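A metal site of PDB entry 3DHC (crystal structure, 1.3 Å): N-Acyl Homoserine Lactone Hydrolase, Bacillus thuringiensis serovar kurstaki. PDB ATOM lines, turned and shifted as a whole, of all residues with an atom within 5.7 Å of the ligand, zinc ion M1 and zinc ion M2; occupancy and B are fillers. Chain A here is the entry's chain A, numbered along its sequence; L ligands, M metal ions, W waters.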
ATOM      1  N   CYS A  18      23.064  11.583   6.224  1.00  0.00           N
ATOM      2  CA  CYS A  18      22.798  10.966   4.924  1.00  0.00           C
ATOM      3  C   CYS A  18      21.313  10.749   4.770  1.00  0.00           C
ATOM      4  O   CYS A  18      20.674  10.222   5.680  1.00  0.00           O
ATOM      5  CB  CYS A  18      23.587   9.655   4.837  1.00  0.00           C
ATOM      6  SG  CYS A  18      23.555   8.966   3.157  1.00  0.00           S
ATOM      7  N   MET A  19      20.766  11.126   3.608  1.00  0.00           N
ATOM      8  CA  MET A  19      19.341  10.782   3.321  1.00  0.00           C
ATOM      9  C   MET A  19      19.285   9.375   2.806  1.00  0.00           C
ATOM     10  O   MET A  19      20.080   8.973   1.926  1.00  0.00           O
ATOM     11  CB  MET A  19      18.802  11.710   2.256  1.00  0.00           C
ATOM     12  CG  MET A  19      19.162  13.111   2.619  1.00  0.00           C
ATOM     13  SD  MET A  19      17.859  14.205   2.238  1.00  0.00           S
ATOM     14  CE  MET A  19      16.412  13.426   2.990  1.00  0.00           C
ATOM     15  N   LEU A  20      18.340   8.622   3.354  1.00  0.00           N
ATOM     16  CA  LEU A  20      18.124   7.260   2.928  1.00  0.00           C
ATOM     17  C   LEU A  20      16.623   7.060   2.778  1.00  0.00           C
ATOM     18  O   LEU A  20      15.885   7.541   3.575  1.00  0.00           O
ATOM     19  CB  LEU A  20      18.736   6.326   3.989  1.00  0.00           C
ATOM     20  CG  LEU A  20      18.683   4.823   3.789  1.00  0.00           C
ATOM     21  CD1 LEU A  20      19.536   4.478   2.537  1.00  0.00           C
ATOM     22  CD2 LEU A  20      19.190   4.076   5.005  1.00  0.00           C
ATOM     23  N   LEU A  37      19.322  10.796   8.140  1.00  0.00           N
ATOM     24  CA  LEU A  37      19.825   9.960   9.222  1.00  0.00           C
ATOM     25  C   LEU A  37      21.212  10.427   9.646  1.00  0.00           C
ATOM     26  O   LEU A  37      22.000  10.968   8.841  1.00  0.00           O
ATOM     27  CB  LEU A  37      20.001   8.510   8.698  1.00  0.00           C
ATOM     28  CG  LEU A  37      18.714   7.818   8.262  1.00  0.00           C
ATOM     29  CD1 LEU A  37      18.980   6.435   7.701  1.00  0.00           C
ATOM     30  CD2 LEU A  37      17.736   7.790   9.410  1.00  0.00           C
ATOM     31  N   PRO A  38      21.558  10.184  10.926  1.00  0.00           N
ATOM     32  CA  PRO A  38      22.886  10.616  11.426  1.00  0.00           C
ATOM     33  C   PRO A  38      23.963   9.696  10.956  1.00  0.00           C
ATOM     34  O   PRO A  38      23.718   8.461  10.858  1.00  0.00           O
ATOM     35  CB  PRO A  38      22.730  10.525  12.940  1.00  0.00           C
ATOM     36  CG  PRO A  38      21.688   9.403  13.124  1.00  0.00           C
ATOM     37  CD  PRO A  38      20.720   9.557  11.972  1.00  0.00           C
ATOM     38  N   VAL A  39      25.145  10.242  10.665  1.00  0.00           N
ATOM     39  CA  VAL A  39      26.350   9.423  10.477  1.00  0.00           C
ATOM     40  C   VAL A  39      27.243   9.667  11.692  1.00  0.00           C
ATOM     41  O   VAL A  39      27.434  10.837  12.113  1.00  0.00           O
ATOM     42  CB  VAL A  39      27.087   9.828   9.178  1.00  0.00           C
ATOM     43  CG1 VAL A  39      28.473   9.129   9.046  1.00  0.00           C
ATOM     44  CG2 VAL A  39      26.208   9.536   7.953  1.00  0.00           C
ATOM     45  N   ILE A  77      20.134   7.302  -1.874  1.00  0.00           N
ATOM     46  CA  ILE A  77      21.154   7.675  -0.865  1.00  0.00           C
ATOM     47  C   ILE A  77      21.712   9.036  -1.284  1.00  0.00           C
ATOM     48  O   ILE A  77      22.218   9.170  -2.403  1.00  0.00           O
ATOM     49  CB  ILE A  77      22.309   6.622  -0.853  1.00  0.00           C
ATOM     50  CG1 ILE A  77      21.716   5.231  -0.508  1.00  0.00           C
ATOM     51  CG2 ILE A  77      23.357   7.132   0.150  1.00  0.00           C
ATOM     52  CD1 ILE A  77      22.709   4.061  -0.337  1.00  0.00           C
ATOM     53  N   HIS A 108      32.790  -1.483   9.128  1.00  0.00           N
ATOM     54  CA  HIS A 108      32.627  -2.078   7.822  1.00  0.00           C
ATOM     55  C   HIS A 108      33.054  -0.982   6.800  1.00  0.00           C
ATOM     56  O   HIS A 108      33.426   0.129   7.246  1.00  0.00           O
ATOM     57  CB  HIS A 108      31.224  -2.642   7.539  1.00  0.00           C
ATOM     58  CG  HIS A 108      30.118  -1.649   7.580  1.00  0.00           C
ATOM     59  ND1 HIS A 108      29.894  -0.778   8.630  1.00  0.00           N
ATOM     60  CD2 HIS A 108      29.053  -1.503   6.732  1.00  0.00           C
ATOM     61  CE1 HIS A 108      28.726  -0.152   8.431  1.00  0.00           C
ATOM     62  NE2 HIS A 108      28.214  -0.554   7.284  1.00  0.00           N
ATOM     63  N   HIS A 110      31.336   0.319   4.130  1.00  0.00           N
ATOM     64  CA  HIS A 110      30.363   1.193   3.468  1.00  0.00           C
ATOM     65  C   HIS A 110      30.827   2.646   3.524  1.00  0.00           C
ATOM     66  O   HIS A 110      31.573   3.059   4.413  1.00  0.00           O
ATOM     67  CB  HIS A 110      29.009   1.001   4.069  1.00  0.00           C
ATOM     68  CG  HIS A 110      28.401  -0.329   3.697  1.00  0.00           C
ATOM     69  ND1 HIS A 110      27.285  -0.816   4.351  1.00  0.00           N
ATOM     70  CD2 HIS A 110      28.733  -1.255   2.781  1.00  0.00           C
ATOM     71  CE1 HIS A 110      26.942  -1.986   3.827  1.00  0.00           C
ATOM     72  NE2 HIS A 110      27.800  -2.294   2.870  1.00  0.00           N
ATOM     73  N   PHE A 111      30.264   3.454   2.599  1.00  0.00           N
ATOM     74  CA  PHE A 111      30.864   4.765   2.265  1.00  0.00           C
ATOM     75  C   PHE A 111      30.841   5.736   3.400  1.00  0.00           C
ATOM     76  O   PHE A 111      31.701   6.635   3.463  1.00  0.00           O
ATOM     77  CB  PHE A 111      30.271   5.327   0.965  1.00  0.00           C
ATOM     78  CG  PHE A 111      29.047   6.129   1.212  1.00  0.00           C
ATOM     79  CD1 PHE A 111      29.135   7.516   1.195  1.00  0.00           C
ATOM     80  CD2 PHE A 111      27.835   5.536   1.550  1.00  0.00           C
ATOM     81  CE1 PHE A 111      28.048   8.308   1.471  1.00  0.00           C
ATOM     82  CE2 PHE A 111      26.684   6.359   1.888  1.00  0.00           C
ATOM     83  CZ  PHE A 111      26.828   7.725   1.839  1.00  0.00           C
ATOM     84  N   ASP A 112      29.822   5.618   4.273  1.00  0.00           N
ATOM     85  CA  ASP A 112      29.714   6.574   5.377  1.00  0.00           C
ATOM     86  C   ASP A 112      30.372   6.095   6.640  1.00  0.00           C
ATOM     87  O   ASP A 112      30.305   6.802   7.640  1.00  0.00           O
ATOM     88  CB  ASP A 112      28.262   6.947   5.641  1.00  0.00           C
ATOM     89  CG  ASP A 112      27.439   5.796   5.999  1.00  0.00           C
ATOM     90  OD1 ASP A 112      26.721   5.834   7.053  1.00  0.00           O
ATOM     91  OD2 ASP A 112      27.506   4.734   5.289  1.00  0.00           O
ATOM     92  N   HIS A 113      31.069   4.946   6.548  1.00  0.00           N
ATOM     93  CA  HIS A 113      31.859   4.450   7.681  1.00  0.00           C
ATOM     94  C   HIS A 113      33.349   4.392   7.406  1.00  0.00           C
ATOM     95  O   HIS A 113      34.130   4.405   8.367  1.00  0.00           O
ATOM     96  CB  HIS A 113      31.380   3.019   8.020  1.00  0.00           C
ATOM     97  CG  HIS A 113      29.992   3.013   8.505  1.00  0.00           C
ATOM     98  ND1 HIS A 113      29.688   3.112   9.836  1.00  0.00           N
ATOM     99  CD2 HIS A 113      28.826   3.010   7.840  1.00  0.00           C
ATOM    100  CE1 HIS A 113      28.368   3.186   9.968  1.00  0.00           C
ATOM    101  NE2 HIS A 113      27.817   3.093   8.761  1.00  0.00           N
ATOM    102  N   GLU A 140      28.658  -2.075  -4.133  1.00  0.00           N
ATOM    103  CA  GLU A 140      28.222  -1.035  -3.190  1.00  0.00           C
ATOM    104  C   GLU A 140      29.416  -0.391  -2.488  1.00  0.00           C
ATOM    105  O   GLU A 140      29.198   0.447  -1.523  1.00  0.00           O
ATOM    106  CB  GLU A 140      27.252  -1.599  -2.111  1.00  0.00           C
ATOM    107  CG  GLU A 140      27.833  -2.674  -1.161  1.00  0.00           C
ATOM    108  CD  GLU A 140      27.704  -4.109  -1.703  1.00  0.00           C
ATOM    109  OE1 GLU A 140      27.783  -5.046  -0.888  1.00  0.00           O
ATOM    110  OE2 GLU A 140      27.549  -4.330  -2.942  1.00  0.00           O
ATOM    111  N   HIS A 173      24.573  -7.451   7.509  1.00  0.00           N
ATOM    112  CA  HIS A 173      24.350  -6.160   6.831  1.00  0.00           C
ATOM    113  C   HIS A 173      25.420  -5.935   5.732  1.00  0.00           C
ATOM    114  O   HIS A 173      25.130  -5.437   4.633  1.00  0.00           O
ATOM    115  CB  HIS A 173      24.416  -5.051   7.872  1.00  0.00           C
ATOM    116  CG  HIS A 173      24.525  -3.696   7.284  1.00  0.00           C
ATOM    117  ND1 HIS A 173      23.458  -3.063   6.652  1.00  0.00           N
ATOM    118  CD2 HIS A 173      25.581  -2.842   7.195  1.00  0.00           C
ATOM    119  CE1 HIS A 173      23.900  -1.904   6.187  1.00  0.00           C
ATOM    120  NE2 HIS A 173      25.167  -1.742   6.500  1.00  0.00           N
ATOM    121  N   SER A 174      26.667  -6.316   6.049  1.00  0.00           N
ATOM    122  CA  SER A 174      27.753  -6.404   5.055  1.00  0.00           C
ATOM    123  C   SER A 174      28.521  -7.708   5.356  1.00  0.00           C
ATOM    124  O   SER A 174      28.351  -8.313   6.461  1.00  0.00           O
ATOM    125  CB  SER A 174      28.650  -5.182   5.084  1.00  0.00           C
ATOM    126  OG  SER A 174      29.427  -5.178   6.284  1.00  0.00           O
ATOM    127  N   HIS A 177      30.798  -7.194   8.598  1.00  0.00           N
ATOM    128  CA  HIS A 177      30.383  -6.174   9.572  1.00  0.00           C
ATOM    129  C   HIS A 177      30.810  -6.623  10.972  1.00  0.00           C
ATOM    130  O   HIS A 177      30.654  -7.818  11.327  1.00  0.00           O
ATOM    131  CB  HIS A 177      28.850  -5.915   9.494  1.00  0.00           C
ATOM    132  CG  HIS A 177      28.421  -4.882  10.447  1.00  0.00           C
ATOM    133  ND1 HIS A 177      28.305  -3.521  10.181  1.00  0.00           N
ATOM    134  CD2 HIS A 177      28.169  -5.026  11.778  1.00  0.00           C
ATOM    135  CE1 HIS A 177      27.994  -2.865  11.302  1.00  0.00           C
ATOM    136  NE2 HIS A 177      27.897  -3.777  12.283  1.00  0.00           N
ATOM    137  N   ILE A 194      26.445  -0.567  15.641  1.00  0.00           N
ATOM    138  CA  ILE A 194      26.725  -0.045  14.299  1.00  0.00           C
ATOM    139  C   ILE A 194      25.609  -0.558  13.398  1.00  0.00           C
ATOM    140  O   ILE A 194      24.415  -0.478  13.800  1.00  0.00           O
ATOM    141  CB  ILE A 194      28.160  -0.292  13.760  1.00  0.00           C
ATOM    142  CG1 ILE A 194      29.220  -0.236  14.892  1.00  0.00           C
ATOM    143  CG2 ILE A 194      28.432   0.744  12.638  1.00  0.00           C
ATOM    144  CD1 ILE A 194      29.474   1.192  15.482  1.00  0.00           C
ATOM    145  N   ASP A 195      25.935  -1.007  12.191  1.00  0.00           N
ATOM    146  CA  ASP A 195      24.867  -1.315  11.228  1.00  0.00           C
ATOM    147  C   ASP A 195      24.368  -2.750  11.354  1.00  0.00           C
ATOM    148  O   ASP A 195      23.637  -3.219  10.476  1.00  0.00           O
ATOM    149  CB  ASP A 195      25.261  -1.007   9.804  1.00  0.00           C
ATOM    150  CG  ASP A 195      25.340   0.537   9.508  1.00  0.00           C
ATOM    151  OD1 ASP A 195      25.147   1.325  10.442  1.00  0.00           O
ATOM    152  OD2 ASP A 195      25.706   0.851   8.321  1.00  0.00           O
ATOM    153  N   TYR A 198      20.143  -0.667  12.168  1.00  0.00           N
ATOM    154  CA  TYR A 198      20.075   0.774  12.001  1.00  0.00           C
ATOM    155  C   TYR A 198      19.316   1.426  13.140  1.00  0.00           C
ATOM    156  O   TYR A 198      19.692   2.475  13.639  1.00  0.00           O
ATOM    157  CB  TYR A 198      19.342   1.154  10.694  1.00  0.00           C
ATOM    158  CG  TYR A 198      20.099   0.974   9.403  1.00  0.00           C
ATOM    159  CD1 TYR A 198      21.426   0.605   9.342  1.00  0.00           C
ATOM    160  CD2 TYR A 198      19.454   1.172   8.217  1.00  0.00           C
ATOM    161  CE1 TYR A 198      22.045   0.496   8.133  1.00  0.00           C
ATOM    162  CE2 TYR A 198      20.076   1.059   6.983  1.00  0.00           C
ATOM    163  CZ  TYR A 198      21.384   0.725   6.969  1.00  0.00           C
ATOM    164  OH  TYR A 198      22.017   0.672   5.738  1.00  0.00           O
ATOM    165  N   ALA A 210      18.118  -2.678   5.324  1.00  0.00           N
ATOM    166  CA  ALA A 210      19.017  -2.917   4.208  1.00  0.00           C
ATOM    167  C   ALA A 210      20.193  -3.776   4.646  1.00  0.00           C
ATOM    168  O   ALA A 210      20.828  -3.534   5.701  1.00  0.00           O
ATOM    169  CB  ALA A 210      19.546  -1.595   3.686  1.00  0.00           C
ATOM    170  N   GLY A 211      20.561  -4.716   3.795  1.00  0.00           N
ATOM    171  CA  GLY A 211      21.723  -5.549   4.085  1.00  0.00           C
ATOM    172  C   GLY A 211      22.045  -6.509   2.969  1.00  0.00           C
ATOM    173  O   GLY A 211      21.183  -6.883   2.174  1.00  0.00           O
ATOM    174  N   PHE A 212      23.311  -6.915   2.926  1.00  0.00           N
ATOM    175  CA  PHE A 212      23.785  -7.863   1.949  1.00  0.00           C
ATOM    176  C   PHE A 212      23.116  -9.261   2.058  1.00  0.00           C
ATOM    177  O   PHE A 212      22.770  -9.886   1.031  1.00  0.00           O
ATOM    178  CB  PHE A 212      25.308  -7.888   2.063  1.00  0.00           C
ATOM    179  CG  PHE A 212      25.928  -9.236   2.124  1.00  0.00           C
ATOM    180  CD1 PHE A 212      26.252  -9.899   0.959  1.00  0.00           C
ATOM    181  CD2 PHE A 212      26.329  -9.783   3.369  1.00  0.00           C
ATOM    182  CE1 PHE A 212      26.867 -11.138   1.000  1.00  0.00           C
ATOM    183  CE2 PHE A 212      26.937 -11.024   3.421  1.00  0.00           C
ATOM    184  CZ  PHE A 212      27.212 -11.687   2.223  1.00  0.00           C
ATOM    185  N   GLY A 238      22.825   2.044  14.879  1.00  0.00           N
ATOM    186  CA  GLY A 238      23.706   2.724  13.908  1.00  0.00           C
ATOM    187  C   GLY A 238      23.180   4.021  13.253  1.00  0.00           C
ATOM    188  O   GLY A 238      23.984   4.926  12.979  1.00  0.00           O
ATOM    189  N   HIS A 239      21.889   4.097  12.978  1.00  0.00           N
ATOM    190  CA  HIS A 239      21.329   5.267  12.213  1.00  0.00           C
ATOM    191  C   HIS A 239      19.904   5.458  12.688  1.00  0.00           C
ATOM    192  O   HIS A 239      18.959   5.247  11.891  1.00  0.00           O
ATOM    193  CB  HIS A 239      21.301   4.941  10.693  1.00  0.00           C
ATOM    194  CG  HIS A 239      22.658   4.794  10.078  1.00  0.00           C
ATOM    195  ND1 HIS A 239      23.556   5.845   9.926  1.00  0.00           N
ATOM    196  CD2 HIS A 239      23.229   3.716   9.506  1.00  0.00           C
ATOM    197  CE1 HIS A 239      24.640   5.390   9.331  1.00  0.00           C
ATOM    198  NE2 HIS A 239      24.443   4.120   9.031  1.00  0.00           N
HETATM  199  C1  LIG L   1      23.473   3.893   4.933  1.00  0.00           C
HETATM  200  C2  LIG L   1      25.172   1.986   2.232  1.00  0.00           C
HETATM  201  C3  LIG L   1      25.318   2.256   5.367  1.00  0.00           C
HETATM  202  O1  LIG L   1      26.391   2.269   2.326  1.00  0.00           O
HETATM  203  N1  LIG L   1      24.271   2.409   3.110  1.00  0.00           N
HETATM  204  C4  LIG L   1      24.636   3.122   4.328  1.00  0.00           C
HETATM  205  O2  LIG L   1      25.905   2.685   6.267  1.00  0.00           O
HETATM  206  O3  LIG L   1      25.273   1.089   5.307  1.00  0.00           O
HETATM  207  C5  LIG L   1      23.871   5.362   5.209  1.00  0.00           C
HETATM  208  S1  LIG L   1      22.552   6.217   6.091  1.00  0.00           S
HETATM  209  C6  LIG L   1      24.619   1.099   1.131  1.00  0.00           C
HETATM  210  C7  LIG L   1      24.807  -0.404   1.518  1.00  0.00           C
HETATM  211  C8  LIG L   1      23.656  -0.910   2.426  1.00  0.00           C
HETATM  212  C9  LIG L   1      23.455  -2.415   2.723  1.00  0.00           C
HETATM  213  C10 LIG L   1      23.969  -3.291   1.612  1.00  0.00           C
HETATM  214 ZN    ZN M   1      26.419  -0.173   6.227  1.00  0.00          ZN
HETATM  215 ZN    ZN M   2      25.848   2.832   8.223  1.00  0.00          ZN
HETATM  216  O   HOH W   1      28.596   1.897   0.767  1.00  0.00           O
HETATM  217  O   HOH W   2      24.438  -5.417  -0.599  1.00  0.00           O
HETATM  218  O   HOH W   3      21.195   1.412   2.969  1.00  0.00           O
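OH of Tyr 198 lies close to O3 of the ligand, at 3.3 Å.
The backbone NH (N) of Asp 195 lies close to a ring nitrogen (NE2) of His 177 (3.4 Å). The backbone carbonyl oxygen of His 173 sits at hydrogen-bond distance from the backbone NH of Phe 212, at 2.9 Å. ND1 of His 173 sits at hydrogen-bond distance from O of Ala 210, at 2.8 Å. A ring nitrogen (NE2) of His 113 sits close to the side-chain carboxylate of Asp 112 (3.4 Å). N of His 239 is in hydrogen-bond range of O of Tyr 198 (2.8 Å). The backbone carbonyl oxygen (O) of Pro 38 lies within hydrogen-bond range of a ring nitrogen (ND1) of His 239 (2.8 Å). The backbone carbonyl oxygen (O) of Tyr 198 is in hydrogen-bond range of the backbone NH (N) of Gly 238. O of Cys 18 lies within hydrogen-bond range of N of Leu 37 (2.9 Å).
O2 of the ligand lies close to OD2 of Asp 112 (2.8 Å). Residues that only touch the ligand: Cys 18 (3.8 Å), Leu 37 (3.9 Å), Ile 77 (3.8 Å), Phe 111 (3.7 Å), Gly 211 (3.8 Å) and Phe 212 (3.9 Å). Within 4 Å of the ligand: Cys 18, Leu 37, Ile 77, His 108, His 110, Phe 111, Asp 112, His 113, His 173, Asp 195, Tyr 198, Gly 211, Phe 212 and His 239.
Four residues have an atom within 4 Å of zinc ion M1: His 108, His 110, His 173 and Asp 195. The nearest printed residue that does not touch zinc ion M1 is His 113 (4.3 Å).
Merely in contact with zinc ion M2: Asp 112. Within 4 Å of zinc ion M2: Asp 112, His 113, Asp 195 and His 239.
O3 of the ligand binds zinc ion M1, 1.9 Å away. Zinc ion M1 is bound by NE2 of His 173 (2.0 Å). NE2 of His 108 is bound to zinc ion M1, 2.1 Å away. Zinc ion M1 is bound by a ring nitrogen (ND1) of His 110, 2.2 Å away. The side-chain carboxylate (OD2) of Asp 195 binds zinc ion M1, at 2.4 Å. Zinc ion M1 has five donor atoms within binding distance.
Zinc ion M2 is bound by O2 of the ligand (2.0 Å), OD2 of Asp 195 (2.0 Å), NE2 of His 113 (2.1 Å) and NE2 of His 239 (2.1 Å). Zinc ion M2 has four donor atoms within binding distance. Slightly farther from zinc ion M2 lies OD1 of Asp 195 (2.8 Å).
Water W1 lies within hydrogen-bond range of O1 of the ligand (2.7 Å), O of Glu 140 (2.8 Å) and N of Phe 111 (2.9 Å). Water W3 lies within hydrogen-bond range of OH of Tyr 198 (3.0 Å) and N1 of the ligand (3.2 Å).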
